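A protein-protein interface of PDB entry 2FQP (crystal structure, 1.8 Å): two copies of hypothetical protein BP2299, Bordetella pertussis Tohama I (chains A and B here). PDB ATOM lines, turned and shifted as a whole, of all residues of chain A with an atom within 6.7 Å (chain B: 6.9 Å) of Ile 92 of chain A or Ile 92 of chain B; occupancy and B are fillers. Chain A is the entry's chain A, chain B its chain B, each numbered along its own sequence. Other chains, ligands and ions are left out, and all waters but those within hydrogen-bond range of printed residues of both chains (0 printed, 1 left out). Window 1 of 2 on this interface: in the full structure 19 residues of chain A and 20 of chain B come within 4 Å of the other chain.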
ATOM      1  N   VAL A  18      -4.162 -12.207  30.151  1.00  0.00           N
ATOM      2  CA  VAL A  18      -5.075 -11.095  30.465  1.00  0.00           C
ATOM      3  C   VAL A  18      -5.495 -11.093  31.915  1.00  0.00           C
ATOM      4  O   VAL A  18      -5.443 -12.111  32.608  1.00  0.00           O
ATOM      5  CB  VAL A  18      -6.372 -11.144  29.559  1.00  0.00           C
ATOM      6  CG1 VAL A  18      -6.021 -10.905  28.118  1.00  0.00           C
ATOM      7  CG2 VAL A  18      -7.093 -12.451  29.723  1.00  0.00           C
ATOM      8  N   LYS A  19      -5.860  -9.911  32.391  1.00  0.00           N
ATOM      9  CA  LYS A  19      -6.580  -9.738  33.624  1.00  0.00           C
ATOM     10  C   LYS A  19      -7.850  -8.974  33.279  1.00  0.00           C
ATOM     11  O   LYS A  19      -7.781  -7.875  32.752  1.00  0.00           O
ATOM     12  CB  LYS A  19      -5.767  -8.927  34.632  1.00  0.00           C
ATOM     13  CG  LYS A  19      -6.418  -8.849  36.032  1.00  0.00           C
ATOM     14  CD  LYS A  19      -5.615  -7.910  36.917  1.00  0.00           C
ATOM     15  CE  LYS A  19      -6.169  -7.745  38.320  1.00  0.00           C
ATOM     16  NZ  LYS A  19      -5.256  -6.840  39.109  1.00  0.00           N
ATOM     17  N   VAL A  20      -8.994  -9.552  33.601  1.00  0.00           N
ATOM     18  CA  VAL A  20     -10.280  -8.965  33.257  1.00  0.00           C
ATOM     19  C   VAL A  20     -10.985  -8.632  34.549  1.00  0.00           C
ATOM     20  O   VAL A  20     -11.243  -9.506  35.346  1.00  0.00           O
ATOM     21  CB  VAL A  20     -11.137  -9.936  32.415  1.00  0.00           C
ATOM     22  CG1 VAL A  20     -12.473  -9.340  32.071  1.00  0.00           C
ATOM     23  CG2 VAL A  20     -10.405 -10.341  31.171  1.00  0.00           C
ATOM     24  N   THR A  21     -11.319  -7.359  34.723  1.00  0.00           N
ATOM     25  CA  THR A  21     -11.890  -6.852  35.942  1.00  0.00           C
ATOM     26  C   THR A  21     -13.205  -6.138  35.604  1.00  0.00           C
ATOM     27  O   THR A  21     -13.219  -5.306  34.724  1.00  0.00           O
ATOM     28  CB  THR A  21     -10.915  -5.888  36.642  1.00  0.00           C
ATOM     29  OG1 THR A  21      -9.673  -6.574  36.944  1.00  0.00           O
ATOM     30  CG2 THR A  21     -11.522  -5.351  37.950  1.00  0.00           C
ATOM     31  N   MET A  38      -0.614  -1.584  31.903  1.00  0.00           N
ATOM     32  CA  MET A  38      -0.792  -2.379  30.686  1.00  0.00           C
ATOM     33  C   MET A  38      -1.702  -1.734  29.683  1.00  0.00           C
ATOM     34  O   MET A  38      -2.627  -1.013  30.062  1.00  0.00           O
ATOM     35  CB  MET A  38      -1.388  -3.721  31.086  1.00  0.00           C
ATOM     36  CG  MET A  38      -0.401  -4.596  31.780  1.00  0.00           C
ATOM     37  SD  MET A  38      -1.352  -6.163  32.485  1.00  0.00           S
ATOM     38  CE  MET A  38      -1.778  -5.478  34.238  1.00  0.00           C
ATOM     39  N   ASP A  39      -1.482  -1.992  28.394  1.00  0.00           N
ATOM     40  CA  ASP A  39      -2.541  -1.653  27.402  1.00  0.00           C
ATOM     41  C   ASP A  39      -3.834  -2.333  27.862  1.00  0.00           C
ATOM     42  O   ASP A  39      -3.826  -3.445  28.429  1.00  0.00           O
ATOM     43  CB  ASP A  39      -2.197  -2.118  25.989  1.00  0.00           C
ATOM     44  CG  ASP A  39      -0.950  -1.456  25.414  1.00  0.00           C
ATOM     45  OD1 ASP A  39      -0.548  -0.367  25.861  1.00  0.00           O
ATOM     46  OD2 ASP A  39      -0.382  -2.039  24.458  1.00  0.00           O
ATOM     47  N   TYR A  40      -4.957  -1.685  27.616  1.00  0.00           N
ATOM     48  CA  TYR A  40      -6.235  -2.236  28.079  1.00  0.00           C
ATOM     49  C   TYR A  40      -7.386  -1.946  27.147  1.00  0.00           C
ATOM     50  O   TYR A  40      -7.296  -1.054  26.305  1.00  0.00           O
ATOM     51  CB  TYR A  40      -6.538  -1.799  29.524  1.00  0.00           C
ATOM     52  CG  TYR A  40      -6.801  -0.315  29.729  1.00  0.00           C
ATOM     53  CD1 TYR A  40      -5.756   0.602  29.777  1.00  0.00           C
ATOM     54  CD2 TYR A  40      -8.093   0.158  29.920  1.00  0.00           C
ATOM     55  CE1 TYR A  40      -6.000   1.962  30.015  1.00  0.00           C
ATOM     56  CE2 TYR A  40      -8.343   1.521  30.146  1.00  0.00           C
ATOM     57  CZ  TYR A  40      -7.278   2.416  30.201  1.00  0.00           C
ATOM     58  OH  TYR A  40      -7.493   3.800  30.405  1.00  0.00           O
ATOM     59  N   VAL A  41      -8.414  -2.786  27.256  1.00  0.00           N
ATOM     60  CA  VAL A  41      -9.652  -2.643  26.540  1.00  0.00           C
ATOM     61  C   VAL A  41     -10.796  -2.391  27.505  1.00  0.00           C
ATOM     62  O   VAL A  41     -10.865  -3.024  28.519  1.00  0.00           O
ATOM     63  CB  VAL A  41      -9.949  -3.933  25.707  1.00  0.00           C
ATOM     64  CG1 VAL A  41     -11.294  -3.823  25.064  1.00  0.00           C
ATOM     65  CG2 VAL A  41      -8.833  -4.175  24.665  1.00  0.00           C
ATOM     66  N   VAL A  42     -11.661  -1.407  27.203  1.00  0.00           N
ATOM     67  CA  VAL A  42     -12.813  -1.130  28.015  1.00  0.00           C
ATOM     68  C   VAL A  42     -14.032  -1.576  27.224  1.00  0.00           C
ATOM     69  O   VAL A  42     -14.226  -1.117  26.092  1.00  0.00           O
ATOM     70  CB  VAL A  42     -12.897   0.394  28.352  1.00  0.00           C
ATOM     71  CG1 VAL A  42     -14.199   0.744  29.068  1.00  0.00           C
ATOM     72  CG2 VAL A  42     -11.670   0.841  29.152  1.00  0.00           C
ATOM     73  N   VAL A  43     -14.812  -2.494  27.796  1.00  0.00           N
ATOM     74  CA  VAL A  43     -16.124  -2.824  27.255  1.00  0.00           C
ATOM     75  C   VAL A  43     -17.203  -2.277  28.191  1.00  0.00           C
ATOM     76  O   VAL A  43     -17.450  -2.846  29.241  1.00  0.00           O
ATOM     77  CB  VAL A  43     -16.332  -4.362  27.124  1.00  0.00           C
ATOM     78  CG1 VAL A  43     -17.669  -4.630  26.465  1.00  0.00           C
ATOM     79  CG2 VAL A  43     -15.193  -5.041  26.309  1.00  0.00           C
ATOM     80  N   SER A  68     -16.650  -1.000  22.519  1.00  0.00           N
ATOM     81  CA  SER A  68     -15.359  -1.067  23.171  1.00  0.00           C
ATOM     82  C   SER A  68     -14.388  -0.016  22.648  1.00  0.00           C
ATOM     83  O   SER A  68     -14.554   0.571  21.579  1.00  0.00           O
ATOM     84  CB  SER A  68     -14.738  -2.453  23.004  1.00  0.00           C
ATOM     85  OG  SER A  68     -14.267  -2.647  21.691  1.00  0.00           O
ATOM     86  N   THR A  70      -9.885   1.040  23.241  1.00  0.00           N
ATOM     87  CA  THR A  70      -8.608   0.723  23.872  1.00  0.00           C
ATOM     88  C   THR A  70      -7.786   1.974  24.191  1.00  0.00           C
ATOM     89  O   THR A  70      -7.894   2.991  23.509  1.00  0.00           O
ATOM     90  CB  THR A  70      -7.797  -0.292  23.028  1.00  0.00           C
ATOM     91  OG1 THR A  70      -6.658  -0.734  23.785  1.00  0.00           O
ATOM     92  CG2 THR A  70      -7.361   0.289  21.697  1.00  0.00           C
ATOM     93  N   VAL A  90     -16.319  -3.503  31.886  1.00  0.00           N
ATOM     94  CA  VAL A  90     -15.382  -4.585  31.962  1.00  0.00           C
ATOM     95  C   VAL A  90     -14.067  -4.109  31.331  1.00  0.00           C
ATOM     96  O   VAL A  90     -14.055  -3.619  30.199  1.00  0.00           O
ATOM     97  CB  VAL A  90     -15.920  -5.877  31.290  1.00  0.00           C
ATOM     98  CG1 VAL A  90     -14.823  -6.952  31.202  1.00  0.00           C
ATOM     99  CG2 VAL A  90     -17.112  -6.403  32.093  1.00  0.00           C
ATOM    100  N   GLU A  91     -12.996  -4.228  32.107  1.00  0.00           N
ATOM    101  CA  GLU A  91     -11.680  -3.800  31.702  1.00  0.00           C
ATOM    102  C   GLU A  91     -10.778  -5.020  31.475  1.00  0.00           C
ATOM    103  O   GLU A  91     -10.651  -5.873  32.340  1.00  0.00           O
ATOM    104  CB  GLU A  91     -11.077  -2.863  32.764  1.00  0.00           C
ATOM    105  CG  GLU A  91      -9.887  -2.048  32.276  1.00  0.00           C
ATOM    106  CD  GLU A  91      -9.620  -0.828  33.211  1.00  0.00           C
ATOM    107  OE1 GLU A  91      -8.922  -1.007  34.211  1.00  0.00           O
ATOM    108  OE2 GLU A  91     -10.175   0.257  32.962  1.00  0.00           O
ATOM    109  N   ILE A  92     -10.180  -5.093  30.286  1.00  0.00           N
ATOM    110  CA  ILE A  92      -9.339  -6.239  29.873  1.00  0.00           C
ATOM    111  C   ILE A  92      -7.915  -5.747  29.707  1.00  0.00           C
ATOM    112  O   ILE A  92      -7.610  -5.010  28.767  1.00  0.00           O
ATOM    113  CB  ILE A  92      -9.806  -6.867  28.541  1.00  0.00           C
ATOM    114  CG1 ILE A  92     -11.230  -7.388  28.643  1.00  0.00           C
ATOM    115  CG2 ILE A  92      -8.895  -8.037  28.138  1.00  0.00           C
ATOM    116  CD1 ILE A  92     -12.229  -6.572  27.894  1.00  0.00           C
ATOM    117  N   GLU A  93      -7.059  -6.098  30.655  1.00  0.00           N
ATOM    118  CA  GLU A  93      -5.673  -5.643  30.623  1.00  0.00           C
ATOM    119  C   GLU A  93      -4.848  -6.746  29.954  1.00  0.00           C
ATOM    120  O   GLU A  93      -5.012  -7.947  30.256  1.00  0.00           O
ATOM    121  CB  GLU A  93      -5.140  -5.333  32.020  1.00  0.00           C
ATOM    122  CG  GLU A  93      -5.830  -4.193  32.743  1.00  0.00           C
ATOM    123  CD  GLU A  93      -5.179  -3.972  34.064  1.00  0.00           C
ATOM    124  OE1 GLU A  93      -5.507  -4.729  34.999  1.00  0.00           O
ATOM    125  OE2 GLU A  93      -4.293  -3.103  34.154  1.00  0.00           O
ATOM    126  N   ILE A  94      -3.938  -6.326  29.081  1.00  0.00           N
ATOM    127  CA  ILE A  94      -3.146  -7.250  28.275  1.00  0.00           C
ATOM    128  C   ILE A  94      -1.763  -7.369  28.878  1.00  0.00           C
ATOM    129  O   ILE A  94      -1.030  -6.385  28.964  1.00  0.00           O
ATOM    130  CB  ILE A  94      -3.049  -6.739  26.804  1.00  0.00           C
ATOM    131  CG1 ILE A  94      -4.436  -6.438  26.227  1.00  0.00           C
ATOM    132  CG2 ILE A  94      -2.297  -7.723  25.944  1.00  0.00           C
ATOM    133  CD1 ILE A  94      -5.433  -7.545  26.379  1.00  0.00           C
ATOM    134  N   ARG B  17      -2.146  -5.706  19.538  1.00  0.00           N
ATOM    135  CA  ARG B  17      -2.367  -6.543  20.726  1.00  0.00           C
ATOM    136  C   ARG B  17      -3.644  -7.386  20.660  1.00  0.00           C
ATOM    137  O   ARG B  17      -3.684  -8.514  21.172  1.00  0.00           O
ATOM    138  CB  ARG B  17      -2.358  -5.675  21.988  1.00  0.00           C
ATOM    139  CG  ARG B  17      -0.996  -5.019  22.274  1.00  0.00           C
ATOM    140  CD  ARG B  17      -0.058  -5.998  22.971  1.00  0.00           C
ATOM    141  NE  ARG B  17       0.537  -5.388  24.141  1.00  0.00           N
ATOM    142  CZ  ARG B  17       0.980  -6.039  25.209  1.00  0.00           C
ATOM    143  NH1 ARG B  17       0.931  -7.363  25.302  1.00  0.00           N
ATOM    144  NH2 ARG B  17       1.509  -5.340  26.196  1.00  0.00           N
ATOM    145  N   VAL B  18      -4.709  -6.829  20.100  1.00  0.00           N
ATOM    146  CA  VAL B  18      -5.986  -7.510  20.095  1.00  0.00           C
ATOM    147  C   VAL B  18      -6.817  -7.187  18.843  1.00  0.00           C
ATOM    148  O   VAL B  18      -6.566  -6.228  18.152  1.00  0.00           O
ATOM    149  CB  VAL B  18      -6.856  -7.102  21.340  1.00  0.00           C
ATOM    150  CG1 VAL B  18      -6.217  -7.516  22.663  1.00  0.00           C
ATOM    151  CG2 VAL B  18      -7.169  -5.636  21.328  1.00  0.00           C
ATOM    152  N   LYS B  19      -7.792  -8.040  18.560  1.00  0.00           N
ATOM    153  CA  LYS B  19      -8.837  -7.754  17.579  1.00  0.00           C
ATOM    154  C   LYS B  19     -10.168  -7.995  18.337  1.00  0.00           C
ATOM    155  O   LYS B  19     -10.460  -9.083  18.844  1.00  0.00           O
ATOM    156  CB  LYS B  19      -8.724  -8.688  16.360  1.00  0.00           C
ATOM    157  CG  LYS B  19      -9.760  -8.464  15.316  1.00  0.00           C
ATOM    158  CD  LYS B  19      -9.696  -9.637  14.374  1.00  0.00           C
ATOM    159  CE  LYS B  19     -10.546  -9.459  13.184  1.00  0.00           C
ATOM    160  NZ  LYS B  19     -10.193 -10.556  12.221  1.00  0.00           N
ATOM    161  N   VAL B  20     -10.953  -6.933  18.405  1.00  0.00           N
ATOM    162  CA  VAL B  20     -12.229  -6.965  19.112  1.00  0.00           C
ATOM    163  C   VAL B  20     -13.363  -6.851  18.136  1.00  0.00           C
ATOM    164  O   VAL B  20     -13.421  -5.905  17.378  1.00  0.00           O
ATOM    165  CB  VAL B  20     -12.308  -5.798  20.116  1.00  0.00           C
ATOM    166  CG1 VAL B  20     -13.621  -5.859  20.863  1.00  0.00           C
ATOM    167  CG2 VAL B  20     -11.183  -5.867  21.114  1.00  0.00           C
ATOM    168  N   THR B  21     -14.257  -7.844  18.144  1.00  0.00           N
ATOM    169  CA  THR B  21     -15.367  -7.917  17.229  1.00  0.00           C
ATOM    170  C   THR B  21     -16.647  -8.021  18.014  1.00  0.00           C
ATOM    171  O   THR B  21     -16.759  -8.854  18.927  1.00  0.00           O
ATOM    172  CB  THR B  21     -15.256  -9.134  16.291  1.00  0.00           C
ATOM    173  OG1 THR B  21     -13.997  -9.071  15.594  1.00  0.00           O
ATOM    174  CG2 THR B  21     -16.458  -9.190  15.294  1.00  0.00           C
ATOM    175  N   MET B  38      -6.713 -17.807  17.674  1.00  0.00           N
ATOM    176  CA  MET B  38      -6.151 -17.161  18.872  1.00  0.00           C
ATOM    177  C   MET B  38      -7.003 -17.425  20.126  1.00  0.00           C
ATOM    178  O   MET B  38      -8.261 -17.583  20.081  1.00  0.00           O
ATOM    179  CB  MET B  38      -6.051 -15.646  18.673  1.00  0.00           C
ATOM    180  CG  MET B  38      -5.086 -15.143  17.639  1.00  0.00           C
ATOM    181  SD  MET B  38      -5.550 -13.255  17.196  1.00  0.00           S
ATOM    182  CE  MET B  38      -6.908 -13.555  15.731  1.00  0.00           C
ATOM    183  N   ASP B  39      -6.328 -17.419  21.267  1.00  0.00           N
ATOM    184  CA  ASP B  39      -6.984 -17.375  22.547  1.00  0.00           C
ATOM    185  C   ASP B  39      -7.877 -16.141  22.567  1.00  0.00           C
ATOM    186  O   ASP B  39      -7.522 -15.084  22.010  1.00  0.00           O
ATOM    187  CB  ASP B  39      -5.948 -17.219  23.657  1.00  0.00           C
ATOM    188  CG  ASP B  39      -5.163 -18.500  23.947  1.00  0.00           C
ATOM    189  OD1 ASP B  39      -5.462 -19.580  23.412  1.00  0.00           O
ATOM    190  OD2 ASP B  39      -4.217 -18.385  24.732  1.00  0.00           O
ATOM    191  N   TYR B  40      -9.037 -16.240  23.213  1.00  0.00           N
ATOM    192  CA  TYR B  40     -10.001 -15.146  23.156  1.00  0.00           C
ATOM    193  C   TYR B  40     -10.826 -15.044  24.413  1.00  0.00           C
ATOM    194  O   TYR B  40     -10.997 -15.997  25.171  1.00  0.00           O
ATOM    195  CB  TYR B  40     -10.939 -15.205  21.928  1.00  0.00           C
ATOM    196  CG  TYR B  40     -11.878 -16.404  21.837  1.00  0.00           C
ATOM    197  CD1 TYR B  40     -11.396 -17.667  21.471  1.00  0.00           C
ATOM    198  CD2 TYR B  40     -13.238 -16.269  22.110  1.00  0.00           C
ATOM    199  CE1 TYR B  40     -12.237 -18.757  21.379  1.00  0.00           C
ATOM    200  CE2 TYR B  40     -14.116 -17.334  21.991  1.00  0.00           C
ATOM    201  CZ  TYR B  40     -13.606 -18.599  21.635  1.00  0.00           C
ATOM    202  OH  TYR B  40     -14.473 -19.676  21.557  1.00  0.00           O
ATOM    203  N   VAL B  41     -11.350 -13.843  24.611  1.00  0.00           N
ATOM    204  CA  VAL B  41     -12.223 -13.578  25.730  1.00  0.00           C
ATOM    205  C   VAL B  41     -13.594 -13.159  25.176  1.00  0.00           C
ATOM    206  O   VAL B  41     -13.649 -12.422  24.173  1.00  0.00           O
ATOM    207  CB  VAL B  41     -11.676 -12.401  26.564  1.00  0.00           C
ATOM    208  CG1 VAL B  41     -12.640 -12.048  27.669  1.00  0.00           C
ATOM    209  CG2 VAL B  41     -10.337 -12.701  27.198  1.00  0.00           C
ATOM    210  N   VAL B  42     -14.672 -13.653  25.782  1.00  0.00           N
ATOM    211  CA  VAL B  42     -16.035 -13.297  25.396  1.00  0.00           C
ATOM    212  C   VAL B  42     -16.676 -12.453  26.500  1.00  0.00           C
ATOM    213  O   VAL B  42     -16.687 -12.865  27.657  1.00  0.00           O
ATOM    214  CB  VAL B  42     -16.925 -14.559  25.130  1.00  0.00           C
ATOM    215  CG1 VAL B  42     -18.404 -14.164  24.861  1.00  0.00           C
ATOM    216  CG2 VAL B  42     -16.322 -15.399  24.039  1.00  0.00           C
ATOM    217  N   VAL B  43     -17.149 -11.253  26.150  1.00  0.00           N
ATOM    218  CA  VAL B  43     -18.014 -10.479  27.014  1.00  0.00           C
ATOM    219  C   VAL B  43     -19.453 -10.457  26.498  1.00  0.00           C
ATOM    220  O   VAL B  43     -19.782  -9.734  25.523  1.00  0.00           O
ATOM    221  CB  VAL B  43     -17.513  -9.008  27.210  1.00  0.00           C
ATOM    222  CG1 VAL B  43     -18.388  -8.284  28.214  1.00  0.00           C
ATOM    223  CG2 VAL B  43     -16.022  -9.008  27.690  1.00  0.00           C
ATOM    224  N   SER B  68     -17.727 -12.384  31.818  1.00  0.00           N
ATOM    225  CA  SER B  68     -16.786 -12.736  30.801  1.00  0.00           C
ATOM    226  C   SER B  68     -16.177 -14.114  31.047  1.00  0.00           C
ATOM    227  O   SER B  68     -16.188 -14.631  32.158  1.00  0.00           O
ATOM    228  CB  SER B  68     -15.663 -11.707  30.772  1.00  0.00           C
ATOM    229  OG  SER B  68     -14.737 -11.929  31.818  1.00  0.00           O
ATOM    230  N   THR B  70     -13.051 -17.026  29.016  1.00  0.00           N
ATOM    231  CA  THR B  70     -12.012 -17.142  27.993  1.00  0.00           C
ATOM    232  C   THR B  70     -12.009 -18.584  27.461  1.00  0.00           C
ATOM    233  O   THR B  70     -12.448 -19.537  28.137  1.00  0.00           O
ATOM    234  CB  THR B  70     -10.597 -16.663  28.469  1.00  0.00           C
ATOM    235  OG1 THR B  70      -9.667 -16.616  27.364  1.00  0.00           O
ATOM    236  CG2 THR B  70     -10.043 -17.539  29.571  1.00  0.00           C
ATOM    237  N   VAL B  90     -19.334  -9.428  22.666  1.00  0.00           N
ATOM    238  CA  VAL B  90     -18.073  -8.867  22.196  1.00  0.00           C
ATOM    239  C   VAL B  90     -16.985  -9.918  22.392  1.00  0.00           C
ATOM    240  O   VAL B  90     -16.856 -10.508  23.448  1.00  0.00           O
ATOM    241  CB  VAL B  90     -17.784  -7.564  22.956  1.00  0.00           C
ATOM    242  CG1 VAL B  90     -16.378  -7.027  22.641  1.00  0.00           C
ATOM    243  CG2 VAL B  90     -18.858  -6.483  22.645  1.00  0.00           C
ATOM    244  N   GLU B  91     -16.194 -10.137  21.360  1.00  0.00           N
ATOM    245  CA  GLU B  91     -15.132 -11.116  21.386  1.00  0.00           C
ATOM    246  C   GLU B  91     -13.783 -10.399  21.257  1.00  0.00           C
ATOM    247  O   GLU B  91     -13.587  -9.580  20.334  1.00  0.00           O
ATOM    248  CB  GLU B  91     -15.364 -12.109  20.257  1.00  0.00           C
ATOM    249  CG  GLU B  91     -14.523 -13.334  20.293  1.00  0.00           C
ATOM    250  CD  GLU B  91     -15.108 -14.440  19.378  1.00  0.00           C
ATOM    251  OE1 GLU B  91     -16.074 -15.146  19.777  1.00  0.00           O
ATOM    252  OE2 GLU B  91     -14.557 -14.569  18.278  1.00  0.00           O
ATOM    253  N   ILE B  92     -12.903 -10.634  22.215  1.00  0.00           N
ATOM    254  CA  ILE B  92     -11.569 -10.055  22.219  1.00  0.00           C
ATOM    255  C   ILE B  92     -10.545 -11.160  21.911  1.00  0.00           C
ATOM    256  O   ILE B  92     -10.255 -11.973  22.776  1.00  0.00           O
ATOM    257  CB  ILE B  92     -11.253  -9.383  23.596  1.00  0.00           C
ATOM    258  CG1 ILE B  92     -12.330  -8.355  23.937  1.00  0.00           C
ATOM    259  CG2 ILE B  92      -9.843  -8.781  23.625  1.00  0.00           C
ATOM    260  CD1 ILE B  92     -13.317  -8.882  24.950  1.00  0.00           C
ATOM    261  N   GLU B  93     -10.005 -11.156  20.703  1.00  0.00           N
ATOM    262  CA  GLU B  93      -8.939 -12.118  20.327  1.00  0.00           C
ATOM    263  C   GLU B  93      -7.576 -11.555  20.677  1.00  0.00           C
ATOM    264  O   GLU B  93      -7.247 -10.431  20.344  1.00  0.00           O
ATOM    265  CB  GLU B  93      -8.996 -12.460  18.854  1.00  0.00           C
ATOM    266  CG  GLU B  93     -10.267 -13.104  18.432  1.00  0.00           C
ATOM    267  CD  GLU B  93     -10.265 -13.438  16.972  1.00  0.00           C
ATOM    268  OE1 GLU B  93      -9.744 -14.523  16.610  1.00  0.00           O
ATOM    269  OE2 GLU B  93     -10.713 -12.584  16.187  1.00  0.00           O
ATOM    270  N   ILE B  94      -6.789 -12.351  21.369  1.00  0.00           N
ATOM    271  CA  ILE B  94      -5.465 -11.932  21.786  1.00  0.00           C
ATOM    272  C   ILE B  94      -4.379 -12.312  20.763  1.00  0.00           C
ATOM    273  O   ILE B  94      -4.165 -13.494  20.519  1.00  0.00           O
ATOM    274  CB  ILE B  94      -5.119 -12.553  23.130  1.00  0.00           C
ATOM    275  CG1 ILE B  94      -6.261 -12.390  24.142  1.00  0.00           C
ATOM    276  CG2 ILE B  94      -3.769 -11.971  23.615  1.00  0.00           C
ATOM    277  CD1 ILE B  94      -6.580 -10.975  24.516  1.00  0.00           C
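NE of Arg 17 of chain B lies within salt-bridge range of OD2 of Asp 39 of chain A (3.5 Å).
O of Asp 39 of chain A lies within hydrogen-bond range of N of Ile 94 of chain A (3.0 Å). The backbone carbonyl oxygen (O) of Val 41 of chain A lies within hydrogen-bond range of the backbone NH (N) of Ile 92 of chain A (2.8 Å). The backbone carbonyl oxygen of Asp 39 of chain B lies within hydrogen-bond range of the backbone NH of Ile 94 of chain B, at 2.9 Å. O of Val 41 of chain B lies within hydrogen-bond range of N of Ile 92 of chain B (2.8 Å).
Among the printed residues, pairs that only touch across the chains: Val 18 of chain A with Ile 94 of chain B, Val 20 of chain A with Ser 68 of chain B, Ser 68 of chain A with Val 20 of chain B, Ile 92 of chain A with Ile 92 of chain B, Ile 94 of chain A with Arg 17 of chain B and Ile 94 of chain A with Val 18 of chain B.
Ile 92 of chain A touches just one residue of chain B: Ile 92. Of chain A, only Ile 92 (3.9 Å) comes within 4 Å of Ile 92 of chain B. Of the printed residues of chain A, Ile 94 of chain B touches Val 18. Printed residues of chain B within 4 Å of Ile 94 of chain A: Arg 17 and Val 18. Printed residues of chain A within 4 Å of Ser 68 of chain B: Val 20 (3.4 Å). Of the printed residues of chain B, Asp 39 of chain A touches Arg 17 (3.5 Å). Printed residues of chain B within 4 Å of Val 18 of chain A: Ile 94. The nearest residue of chain B that does not touch Ile 92 of chain A is Val 43 of chain B (4.5 Å).
Of the 17 printed residues of chain A, 6 touch a printed residue of chain B. Hydrophobic or aromatic side chains of chain A within 4 Å of the printed part of chain B: Val 18, Val 20, Ile 92 and Ile 94. Hydrophobic or aromatic side chains of chain B that line the printed part of chain A: Val 18, Val 20, Ile 92 and Ile 94.
Val 18 of chain A touches Ile 94 of chain B, and with the chains exchanged Ile 94 of chain A touches Val 18 of chain B. Val 20 of chain A touches Ser 68 of chain B, and with the chains exchanged Ser 68 of chain A touches Val 20 of chain B. Ile 92 of chain B touches its own counterpart, Ile 92 of chain A. Positions printed for both chains: 18, 19, 20, 21, 38, 39, 40, 41, 42, 43, 68, 70, 90, 91, 92, 93 and 94. Of the 7 pairs that touch across the chains among the printed residues, 5 have their exchanged pair printed and touching as well.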
